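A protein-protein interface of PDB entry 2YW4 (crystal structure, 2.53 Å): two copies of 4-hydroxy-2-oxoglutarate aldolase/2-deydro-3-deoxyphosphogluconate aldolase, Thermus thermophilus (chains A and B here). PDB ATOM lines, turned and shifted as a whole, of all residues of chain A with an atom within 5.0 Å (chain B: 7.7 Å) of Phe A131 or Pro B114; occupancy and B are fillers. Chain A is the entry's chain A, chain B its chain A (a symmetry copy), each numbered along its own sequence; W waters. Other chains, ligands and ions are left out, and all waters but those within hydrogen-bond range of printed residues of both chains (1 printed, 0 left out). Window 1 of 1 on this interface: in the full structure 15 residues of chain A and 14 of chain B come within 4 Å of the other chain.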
ATOM      1  N   PRO A  90       3.124  -6.831   0.209  1.00  0.00           N
ATOM      2  CA  PRO A  90       3.286  -5.346   0.136  1.00  0.00           C
ATOM      3  C   PRO A  90       2.910  -4.606   1.381  1.00  0.00           C
ATOM      4  O   PRO A  90       3.544  -3.607   1.651  1.00  0.00           O
ATOM      5  CB  PRO A  90       2.404  -4.916  -1.002  1.00  0.00           C
ATOM      6  CG  PRO A  90       1.403  -6.124  -1.234  1.00  0.00           C
ATOM      7  CD  PRO A  90       2.129  -7.347  -0.742  1.00  0.00           C
ATOM      8  N   GLY A  91       1.929  -5.111   2.151  1.00  0.00           N
ATOM      9  CA  GLY A  91       1.476  -4.503   3.471  1.00  0.00           C
ATOM     10  C   GLY A  91       1.393  -5.643   4.447  1.00  0.00           C
ATOM     11  O   GLY A  91       1.715  -6.822   4.124  1.00  0.00           O
ATOM     12  N   VAL A 111       6.047  -2.315   5.416  1.00  0.00           N
ATOM     13  CA  VAL A 111       5.600  -1.220   6.259  1.00  0.00           C
ATOM     14  C   VAL A 111       6.102   0.077   5.704  1.00  0.00           C
ATOM     15  O   VAL A 111       6.975   0.094   4.819  1.00  0.00           O
ATOM     16  CB  VAL A 111       6.044  -1.296   7.716  1.00  0.00           C
ATOM     17  CG1 VAL A 111       5.455  -2.473   8.410  1.00  0.00           C
ATOM     18  CG2 VAL A 111       7.536  -1.165   7.869  1.00  0.00           C
ATOM     19  N   LEU A 112       5.529   1.160   6.228  1.00  0.00           N
ATOM     20  CA  LEU A 112       5.937   2.542   5.879  1.00  0.00           C
ATOM     21  C   LEU A 112       6.017   3.515   7.015  1.00  0.00           C
ATOM     22  O   LEU A 112       7.028   4.175   7.146  1.00  0.00           O
ATOM     23  CB  LEU A 112       4.954   3.139   4.873  1.00  0.00           C
ATOM     24  CG  LEU A 112       5.134   2.597   3.446  1.00  0.00           C
ATOM     25  CD1 LEU A 112       4.075   3.502   2.758  1.00  0.00           C
ATOM     26  CD2 LEU A 112       6.560   2.962   2.894  1.00  0.00           C
ATOM     27  N   LYS A 129       9.717  -5.294   5.314  1.00  0.00           N
ATOM     28  CA  LYS A 129       9.795  -4.645   4.013  1.00  0.00           C
ATOM     29  C   LYS A 129       9.496  -3.098   4.165  1.00  0.00           C
ATOM     30  O   LYS A 129       8.695  -2.700   5.003  1.00  0.00           O
ATOM     31  CB  LYS A 129       8.820  -5.349   3.043  1.00  0.00           C
ATOM     32  CG  LYS A 129       8.897  -4.863   1.617  1.00  0.00           C
ATOM     33  CD  LYS A 129       8.176  -5.823   0.701  1.00  0.00           C
ATOM     34  CE  LYS A 129       7.564  -5.044  -0.437  1.00  0.00           C
ATOM     35  NZ  LYS A 129       7.862  -5.795  -1.656  1.00  0.00           N
ATOM     36  N   PHE A 130      10.186  -2.235   3.408  1.00  0.00           N
ATOM     37  CA  PHE A 130       9.832  -0.858   3.362  1.00  0.00           C
ATOM     38  C   PHE A 130       9.398  -0.574   1.929  1.00  0.00           C
ATOM     39  O   PHE A 130      10.243  -0.603   1.010  1.00  0.00           O
ATOM     40  CB  PHE A 130      10.962   0.004   3.825  1.00  0.00           C
ATOM     41  CG  PHE A 130      10.585   1.459   3.869  1.00  0.00           C
ATOM     42  CD1 PHE A 130       9.926   1.977   4.969  1.00  0.00           C
ATOM     43  CD2 PHE A 130      10.875   2.313   2.800  1.00  0.00           C
ATOM     44  CE1 PHE A 130       9.491   3.333   5.045  1.00  0.00           C
ATOM     45  CE2 PHE A 130      10.486   3.654   2.838  1.00  0.00           C
ATOM     46  CZ  PHE A 130       9.781   4.183   3.998  1.00  0.00           C
ATOM     47  N   PHE A 131       8.093  -0.375   1.703  1.00  0.00           N
ATOM     48  CA  PHE A 131       7.575  -0.384   0.337  1.00  0.00           C
ATOM     49  C   PHE A 131       6.330   0.548   0.255  1.00  0.00           C
ATOM     50  O   PHE A 131       5.437   0.432   1.069  1.00  0.00           O
ATOM     51  CB  PHE A 131       7.306  -1.863  -0.173  1.00  0.00           C
ATOM     52  CG  PHE A 131       6.430  -1.941  -1.439  1.00  0.00           C
ATOM     53  CD1 PHE A 131       7.017  -1.864  -2.699  1.00  0.00           C
ATOM     54  CD2 PHE A 131       5.034  -2.023  -1.338  1.00  0.00           C
ATOM     55  CE1 PHE A 131       6.261  -1.825  -3.845  1.00  0.00           C
ATOM     56  CE2 PHE A 131       4.210  -2.032  -2.461  1.00  0.00           C
ATOM     57  CZ  PHE A 131       4.812  -1.914  -3.768  1.00  0.00           C
ATOM     58  N   PRO A 132       6.228   1.429  -0.768  1.00  0.00           N
ATOM     59  CA  PRO A 132       7.258   1.547  -1.883  1.00  0.00           C
ATOM     60  C   PRO A 132       8.390   2.488  -1.488  1.00  0.00           C
ATOM     61  O   PRO A 132       8.157   3.714  -1.118  1.00  0.00           O
ATOM     62  CB  PRO A 132       6.434   2.085  -3.093  1.00  0.00           C
ATOM     63  CG  PRO A 132       5.441   2.958  -2.447  1.00  0.00           C
ATOM     64  CD  PRO A 132       5.051   2.277  -1.034  1.00  0.00           C
ATOM     65  N   ALA A 133       9.602   1.945  -1.548  1.00  0.00           N
ATOM     66  CA  ALA A 133      10.683   2.701  -0.979  1.00  0.00           C
ATOM     67  C   ALA A 133      10.935   4.095  -1.686  1.00  0.00           C
ATOM     68  O   ALA A 133      11.095   5.142  -1.027  1.00  0.00           O
ATOM     69  CB  ALA A 133      11.889   1.842  -0.889  1.00  0.00           C
ATOM     70  N   PHE A 136       8.615   7.060  -1.287  1.00  0.00           N
ATOM     71  CA  PHE A 136       8.465   7.448   0.106  1.00  0.00           C
ATOM     72  C   PHE A 136       9.797   7.862   0.679  1.00  0.00           C
ATOM     73  O   PHE A 136       9.913   8.162   1.890  1.00  0.00           O
ATOM     74  CB  PHE A 136       7.795   6.352   0.870  1.00  0.00           C
ATOM     75  CG  PHE A 136       6.333   6.332   0.663  1.00  0.00           C
ATOM     76  CD1 PHE A 136       5.524   7.287   1.247  1.00  0.00           C
ATOM     77  CD2 PHE A 136       5.750   5.425  -0.142  1.00  0.00           C
ATOM     78  CE1 PHE A 136       4.099   7.320   1.053  1.00  0.00           C
ATOM     79  CE2 PHE A 136       4.279   5.410  -0.335  1.00  0.00           C
ATOM     80  CZ  PHE A 136       3.470   6.364   0.290  1.00  0.00           C
ATOM     81  N   THR A 157      12.364  -1.869  -1.008  1.00  0.00           N
ATOM     82  CA  THR A 157      12.029  -2.338  -2.356  1.00  0.00           C
ATOM     83  C   THR A 157      11.051  -1.308  -2.905  1.00  0.00           C
ATOM     84  O   THR A 157      10.358  -0.657  -2.127  1.00  0.00           O
ATOM     85  CB  THR A 157      11.222  -3.664  -2.309  1.00  0.00           C
ATOM     86  OG1 THR A 157      11.962  -4.679  -1.584  1.00  0.00           O
ATOM     87  CG2 THR A 157      10.916  -4.130  -3.727  1.00  0.00           C
ATOM     88  N   GLY A 158      10.957  -1.206  -4.235  1.00  0.00           N
ATOM     89  CA  GLY A 158      10.051  -0.292  -4.849  1.00  0.00           C
ATOM     90  C   GLY A 158      10.693   0.923  -5.467  1.00  0.00           C
ATOM     91  O   GLY A 158      10.867   2.005  -4.764  1.00  0.00           O
ATOM     92  N   VAL B 111      -6.746   6.456   1.169  1.00  0.00           N
ATOM     93  CA  VAL B 111      -5.664   5.601   1.629  1.00  0.00           C
ATOM     94  C   VAL B 111      -4.357   6.141   1.139  1.00  0.00           C
ATOM     95  O   VAL B 111      -4.321   7.024   0.265  1.00  0.00           O
ATOM     96  CB  VAL B 111      -5.753   4.145   1.184  1.00  0.00           C
ATOM     97  CG1 VAL B 111      -6.943   3.464   1.763  1.00  0.00           C
ATOM     98  CG2 VAL B 111      -5.608   3.988  -0.305  1.00  0.00           C
ATOM     99  N   LEU B 112      -3.286   5.605   1.723  1.00  0.00           N
ATOM    100  CA  LEU B 112      -1.895   5.938   1.329  1.00  0.00           C
ATOM    101  C   LEU B 112      -0.935   4.791   1.260  1.00  0.00           C
ATOM    102  O   LEU B 112      -0.266   4.652   0.257  1.00  0.00           O
ATOM    103  CB  LEU B 112      -1.299   6.939   2.317  1.00  0.00           C
ATOM    104  CG  LEU B 112      -1.822   8.372   2.130  1.00  0.00           C
ATOM    105  CD1 LEU B 112      -0.920   9.051   3.198  1.00  0.00           C
ATOM    106  CD2 LEU B 112      -1.437   8.918   0.707  1.00  0.00           C
ATOM    107  N   THR B 113      -0.909   3.949   2.310  1.00  0.00           N
ATOM    108  CA  THR B 113       0.032   2.847   2.451  1.00  0.00           C
ATOM    109  C   THR B 113      -0.514   1.555   1.937  1.00  0.00           C
ATOM    110  O   THR B 113      -1.730   1.348   1.963  1.00  0.00           O
ATOM    111  CB  THR B 113       0.557   2.671   3.947  1.00  0.00           C
ATOM    112  OG1 THR B 113      -0.405   1.933   4.736  1.00  0.00           O
ATOM    113  CG2 THR B 113       0.953   4.074   4.619  1.00  0.00           C
ATOM    114  N   PRO B 114       0.391   0.651   1.484  1.00  0.00           N
ATOM    115  CA  PRO B 114      -0.051  -0.687   1.106  1.00  0.00           C
ATOM    116  C   PRO B 114      -0.969  -1.338   2.160  1.00  0.00           C
ATOM    117  O   PRO B 114      -2.053  -1.847   1.790  1.00  0.00           O
ATOM    118  CB  PRO B 114       1.231  -1.443   1.000  1.00  0.00           C
ATOM    119  CG  PRO B 114       2.246  -0.361   0.530  1.00  0.00           C
ATOM    120  CD  PRO B 114       1.847   0.867   1.280  1.00  0.00           C
ATOM    121  N   THR B 115      -0.576  -1.346   3.436  1.00  0.00           N
ATOM    122  CA  THR B 115      -1.375  -1.870   4.537  1.00  0.00           C
ATOM    123  C   THR B 115      -2.787  -1.245   4.534  1.00  0.00           C
ATOM    124  O   THR B 115      -3.781  -1.950   4.589  1.00  0.00           O
ATOM    125  CB  THR B 115      -0.692  -1.570   5.882  1.00  0.00           C
ATOM    126  OG1 THR B 115       0.644  -2.154   5.866  1.00  0.00           O
ATOM    127  CG2 THR B 115      -1.458  -2.244   7.064  1.00  0.00           C
ATOM    128  N   GLU B 116      -2.880   0.077   4.373  1.00  0.00           N
ATOM    129  CA  GLU B 116      -4.179   0.744   4.314  1.00  0.00           C
ATOM    130  C   GLU B 116      -4.993   0.217   3.176  1.00  0.00           C
ATOM    131  O   GLU B 116      -6.194   0.014   3.333  1.00  0.00           O
ATOM    132  CB  GLU B 116      -4.023   2.237   4.197  1.00  0.00           C
ATOM    133  CG  GLU B 116      -3.511   2.735   5.602  1.00  0.00           C
ATOM    134  CD  GLU B 116      -3.251   4.279   5.612  1.00  0.00           C
ATOM    135  OE1 GLU B 116      -3.169   4.977   4.536  1.00  0.00           O
ATOM    136  OE2 GLU B 116      -3.192   4.833   6.714  1.00  0.00           O
ATOM    137  N   VAL B 117      -4.337   0.002   2.045  1.00  0.00           N
ATOM    138  CA  VAL B 117      -4.964  -0.599   0.853  1.00  0.00           C
ATOM    139  C   VAL B 117      -5.563  -1.965   1.179  1.00  0.00           C
ATOM    140  O   VAL B 117      -6.786  -2.104   0.862  1.00  0.00           O
ATOM    141  CB  VAL B 117      -4.000  -0.649  -0.441  1.00  0.00           C
ATOM    142  CG1 VAL B 117      -4.625  -1.488  -1.665  1.00  0.00           C
ATOM    143  CG2 VAL B 117      -3.567   0.719  -0.797  1.00  0.00           C
ATOM    144  N   GLU B 118      -4.814  -2.894   1.828  1.00  0.00           N
ATOM    145  CA  GLU B 118      -5.373  -4.185   2.179  1.00  0.00           C
ATOM    146  C   GLU B 118      -6.597  -4.027   3.086  1.00  0.00           C
ATOM    147  O   GLU B 118      -7.630  -4.765   2.919  1.00  0.00           O
ATOM    148  CB  GLU B 118      -4.332  -5.112   2.853  1.00  0.00           C
ATOM    149  CG  GLU B 118      -3.076  -5.343   1.936  1.00  0.00           C
ATOM    150  CD  GLU B 118      -3.331  -6.382   0.817  1.00  0.00           C
ATOM    151  OE1 GLU B 118      -4.529  -6.701   0.512  1.00  0.00           O
ATOM    152  OE2 GLU B 118      -2.328  -6.967   0.302  1.00  0.00           O
ATOM    153  N   ARG B 119      -6.524  -3.086   4.049  1.00  0.00           N
ATOM    154  CA  ARG B 119      -7.507  -3.007   5.084  1.00  0.00           C
ATOM    155  C   ARG B 119      -8.779  -2.638   4.286  1.00  0.00           C
ATOM    156  O   ARG B 119      -9.782  -3.354   4.355  1.00  0.00           O
ATOM    157  CB  ARG B 119      -7.112  -1.872   6.022  1.00  0.00           C
ATOM    158  CG  ARG B 119      -7.222  -2.040   7.522  1.00  0.00           C
ATOM    159  CD  ARG B 119      -8.619  -1.668   7.954  1.00  0.00           C
ATOM    160  NE  ARG B 119      -8.380  -0.437   8.710  1.00  0.00           N
ATOM    161  CZ  ARG B 119      -9.158   0.226   9.589  1.00  0.00           C
ATOM    162  NH1 ARG B 119     -10.402  -0.120   9.950  1.00  0.00           N
ATOM    163  NH2 ARG B 119      -8.615   1.320  10.110  1.00  0.00           N
ATOM    164  N   ALA B 120      -8.758  -1.564   3.502  1.00  0.00           N
ATOM    165  CA  ALA B 120      -9.903  -1.184   2.656  1.00  0.00           C
ATOM    166  C   ALA B 120     -10.442  -2.351   1.831  1.00  0.00           C
ATOM    167  O   ALA B 120     -11.693  -2.558   1.761  1.00  0.00           O
ATOM    168  CB  ALA B 120      -9.565   0.026   1.672  1.00  0.00           C
ATOM    169  N   LEU B 121      -9.498  -3.069   1.179  1.00  0.00           N
ATOM    170  CA  LEU B 121      -9.871  -4.158   0.313  1.00  0.00           C
ATOM    171  C   LEU B 121     -10.691  -5.157   1.117  1.00  0.00           C
ATOM    172  O   LEU B 121     -11.765  -5.661   0.658  1.00  0.00           O
ATOM    173  CB  LEU B 121      -8.629  -4.892  -0.217  1.00  0.00           C
ATOM    174  CG  LEU B 121      -8.270  -4.546  -1.690  1.00  0.00           C
ATOM    175  CD1 LEU B 121      -6.943  -5.246  -2.116  1.00  0.00           C
ATOM    176  CD2 LEU B 121      -9.388  -4.924  -2.640  1.00  0.00           C
ATOM    177  N   LEU B 128     -10.478   3.500  -4.332  1.00  0.00           N
ATOM    178  CA  LEU B 128      -9.934   4.236  -3.149  1.00  0.00           C
ATOM    179  C   LEU B 128      -9.396   5.649  -3.422  1.00  0.00           C
ATOM    180  O   LEU B 128      -8.782   5.914  -4.423  1.00  0.00           O
ATOM    181  CB  LEU B 128      -8.891   3.383  -2.397  1.00  0.00           C
ATOM    182  CG  LEU B 128      -9.233   1.892  -2.308  1.00  0.00           C
ATOM    183  CD1 LEU B 128      -8.082   0.937  -1.815  1.00  0.00           C
ATOM    184  CD2 LEU B 128     -10.606   1.579  -1.592  1.00  0.00           C
ATOM    185  N   PHE B 130      -6.602   8.458  -2.972  1.00  0.00           N
ATOM    186  CA  PHE B 130      -5.228   8.489  -2.603  1.00  0.00           C
ATOM    187  C   PHE B 130      -4.932   9.919  -2.167  1.00  0.00           C
ATOM    188  O   PHE B 130      -4.941  10.837  -3.014  1.00  0.00           O
ATOM    189  CB  PHE B 130      -4.359   8.015  -3.723  1.00  0.00           C
ATOM    190  CG  PHE B 130      -2.909   7.955  -3.332  1.00  0.00           C
ATOM    191  CD1 PHE B 130      -2.410   6.850  -2.666  1.00  0.00           C
ATOM    192  CD2 PHE B 130      -2.040   9.014  -3.613  1.00  0.00           C
ATOM    193  CE1 PHE B 130      -1.059   6.760  -2.217  1.00  0.00           C
ATOM    194  CE2 PHE B 130      -0.703   8.961  -3.211  1.00  0.00           C
ATOM    195  CZ  PHE B 130      -0.194   7.796  -2.499  1.00  0.00           C
ATOM    196  N   VAL B 141       3.735   6.480  -6.572  1.00  0.00           N
ATOM    197  CA  VAL B 141       3.098   5.547  -5.667  1.00  0.00           C
ATOM    198  C   VAL B 141       2.000   4.711  -6.400  1.00  0.00           C
ATOM    199  O   VAL B 141       2.013   3.460  -6.356  1.00  0.00           O
ATOM    200  CB  VAL B 141       2.602   6.204  -4.392  1.00  0.00           C
ATOM    201  CG1 VAL B 141       2.097   5.102  -3.476  1.00  0.00           C
ATOM    202  CG2 VAL B 141       3.756   7.004  -3.706  1.00  0.00           C
ATOM    203  N   ARG B 143       2.061   4.131  -9.350  1.00  0.00           N
ATOM    204  CA  ARG B 143       2.652   3.208 -10.309  1.00  0.00           C
ATOM    205  C   ARG B 143       3.032   1.880  -9.660  1.00  0.00           C
ATOM    206  O   ARG B 143       2.792   0.792 -10.230  1.00  0.00           O
ATOM    207  CB  ARG B 143       3.818   3.863 -11.063  1.00  0.00           C
ATOM    208  CG  ARG B 143       4.548   2.932 -12.170  1.00  0.00           C
ATOM    209  CD  ARG B 143       5.266   3.763 -13.274  1.00  0.00           C
ATOM    210  NE  ARG B 143       5.777   5.119 -12.770  1.00  0.00           N
ATOM    211  CZ  ARG B 143       5.151   6.313 -12.928  1.00  0.00           C
ATOM    212  NH1 ARG B 143       3.971   6.384 -13.539  1.00  0.00           N
ATOM    213  NH2 ARG B 143       5.700   7.442 -12.472  1.00  0.00           N
ATOM    214  N   ALA B 144       3.617   1.945  -8.450  1.00  0.00           N
ATOM    215  CA  ALA B 144       3.938   0.721  -7.647  1.00  0.00           C
ATOM    216  C   ALA B 144       2.634  -0.091  -7.287  1.00  0.00           C
ATOM    217  O   ALA B 144       2.657  -1.327  -7.194  1.00  0.00           O
ATOM    218  CB  ALA B 144       4.683   1.145  -6.408  1.00  0.00           C
ATOM    219  N   TYR B 145       1.490   0.592  -7.076  1.00  0.00           N
ATOM    220  CA  TYR B 145       0.297  -0.118  -6.696  1.00  0.00           C
ATOM    221  C   TYR B 145      -0.346  -0.792  -7.896  1.00  0.00           C
ATOM    222  O   TYR B 145      -1.053  -1.846  -7.724  1.00  0.00           O
ATOM    223  CB  TYR B 145      -0.697   0.840  -6.107  1.00  0.00           C
ATOM    224  CG  TYR B 145      -0.247   1.353  -4.774  1.00  0.00           C
ATOM    225  CD1 TYR B 145       0.971   0.916  -4.188  1.00  0.00           C
ATOM    226  CD2 TYR B 145      -1.008   2.235  -4.054  1.00  0.00           C
ATOM    227  CE1 TYR B 145       1.391   1.380  -2.958  1.00  0.00           C
ATOM    228  CE2 TYR B 145      -0.609   2.622  -2.747  1.00  0.00           C
ATOM    229  CZ  TYR B 145       0.604   2.176  -2.268  1.00  0.00           C
ATOM    230  OH  TYR B 145       1.033   2.593  -1.037  1.00  0.00           O
ATOM    231  N   ALA B 146      -0.143  -0.232  -9.097  1.00  0.00           N
ATOM    232  CA  ALA B 146      -0.633  -0.860 -10.357  1.00  0.00           C
ATOM    233  C   ALA B 146      -0.216  -2.357 -10.495  1.00  0.00           C
ATOM    234  O   ALA B 146      -1.068  -3.195 -10.767  1.00  0.00           O
ATOM    235  CB  ALA B 146      -0.200  -0.037 -11.611  1.00  0.00           C
ATOM    236  N   GLU B 147       1.045  -2.690 -10.218  1.00  0.00           N
ATOM    237  CA  GLU B 147       1.559  -4.033 -10.190  1.00  0.00           C
ATOM    238  C   GLU B 147       1.040  -4.941  -9.033  1.00  0.00           C
ATOM    239  O   GLU B 147       0.640  -6.095  -9.276  1.00  0.00           O
ATOM    240  CB  GLU B 147       3.099  -3.969 -10.096  1.00  0.00           C
ATOM    241  CG  GLU B 147       3.949  -3.166 -11.206  1.00  0.00           C
ATOM    242  CD  GLU B 147       5.488  -2.917 -10.706  1.00  0.00           C
ATOM    243  OE1 GLU B 147       6.011  -3.793  -9.941  1.00  0.00           O
ATOM    244  OE2 GLU B 147       6.158  -1.860 -11.032  1.00  0.00           O
ATOM    245  N   VAL B 148       1.095  -4.460  -7.774  1.00  0.00           N
ATOM    246  CA  VAL B 148       0.827  -5.320  -6.633  1.00  0.00           C
ATOM    247  C   VAL B 148      -0.603  -5.242  -6.147  1.00  0.00           C
ATOM    248  O   VAL B 148      -1.049  -6.169  -5.418  1.00  0.00           O
ATOM    249  CB  VAL B 148       1.801  -5.116  -5.524  1.00  0.00           C
ATOM    250  CG1 VAL B 148       3.180  -5.223  -6.086  1.00  0.00           C
ATOM    251  CG2 VAL B 148       1.680  -3.741  -4.871  1.00  0.00           C
ATOM    252  N   PHE B 149      -1.316  -4.140  -6.518  1.00  0.00           N
ATOM    253  CA  PHE B 149      -2.772  -4.109  -6.318  1.00  0.00           C
ATOM    254  C   PHE B 149      -3.561  -4.001  -7.600  1.00  0.00           C
ATOM    255  O   PHE B 149      -4.320  -3.104  -7.732  1.00  0.00           O
ATOM    256  CB  PHE B 149      -3.176  -3.007  -5.332  1.00  0.00           C
ATOM    257  CG  PHE B 149      -2.430  -3.103  -3.973  1.00  0.00           C
ATOM    258  CD1 PHE B 149      -2.587  -4.252  -3.167  1.00  0.00           C
ATOM    259  CD2 PHE B 149      -1.612  -2.034  -3.520  1.00  0.00           C
ATOM    260  CE1 PHE B 149      -1.967  -4.363  -2.001  1.00  0.00           C
ATOM    261  CE2 PHE B 149      -1.044  -2.086  -2.355  1.00  0.00           C
ATOM    262  CZ  PHE B 149      -1.192  -3.289  -1.554  1.00  0.00           C
HETATM  263  O   HOH W   1      -0.140  -6.642   1.629  1.00  0.00           O
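Of the printed residues of chain B, Pro A90 touches Pro B114 and Phe B149.
Of the printed residues of chain B, Gly A91 touches Pro B114 and Thr B115.
Of chain B, only Pro B114 (3.3 Å) and Val B148 (3.8 Å) come within 4 Å of Phe A131.
Ala A133 touches none of the printed residues of chain B.
Of the printed residues of chain A, Thr B113 touches Leu A112 (3.7 Å).
Of chain A, only Pro A90, Gly A91, Leu A112 and Phe A131 come within 4 Å of Pro B114.
Of the printed residues of chain A, Thr B115 touches Gly A91 (3.5 Å).
Phe B130 touches none of the printed residues of chain A.
Of the printed residues of chain A, Val B148 touches Phe A131 (3.8 Å).
The nearest residue of chain B that does not touch Phe A131 is Ala B144 (4.04 Å).
Positions printed for both chains: 111, 112 and 130.
Water W1 bridges OE2 of Glu B118 (2.6 Å) and N of Gly A91 (2.6 Å).
OG1 of Thr B113 is in hydrogen-bond range of N of Glu B116.
O of Val A111 lies within hydrogen-bond range of N of Phe A131 (3.3 Å).
Pro A90 touches Pro B114.
Phe B149 touches Pro A90.
Gly A91 touches Pro B114 (N to CB, 3.9 Å).
Gly A91 touches Thr B115.
CG2 of Thr B113 touches CD1 of Leu A112, 3.7 Å away.
Leu A112 touches Pro B114 (CD1 to CD, 3.8 Å).
Pro B114 touches Phe A131 (CG to O, 3.3 Å).
CZ of Phe A131 touches CG2 of Val B148, at 3.8 Å.
Pro A132 touches Ala B144 (CB to CB, 3.9 Å).
CE2 of Phe A136 touches CG2 of Val B141, 3.8 Å away.
Hydrophobic or aromatic side chains of chain A that line the printed part of chain B: Pro A90, Leu A112, Phe A131, Pro A132 and Phe A136.
Along chain A the printed residues that touch a printed residue of chain B span positions 90 to 136.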
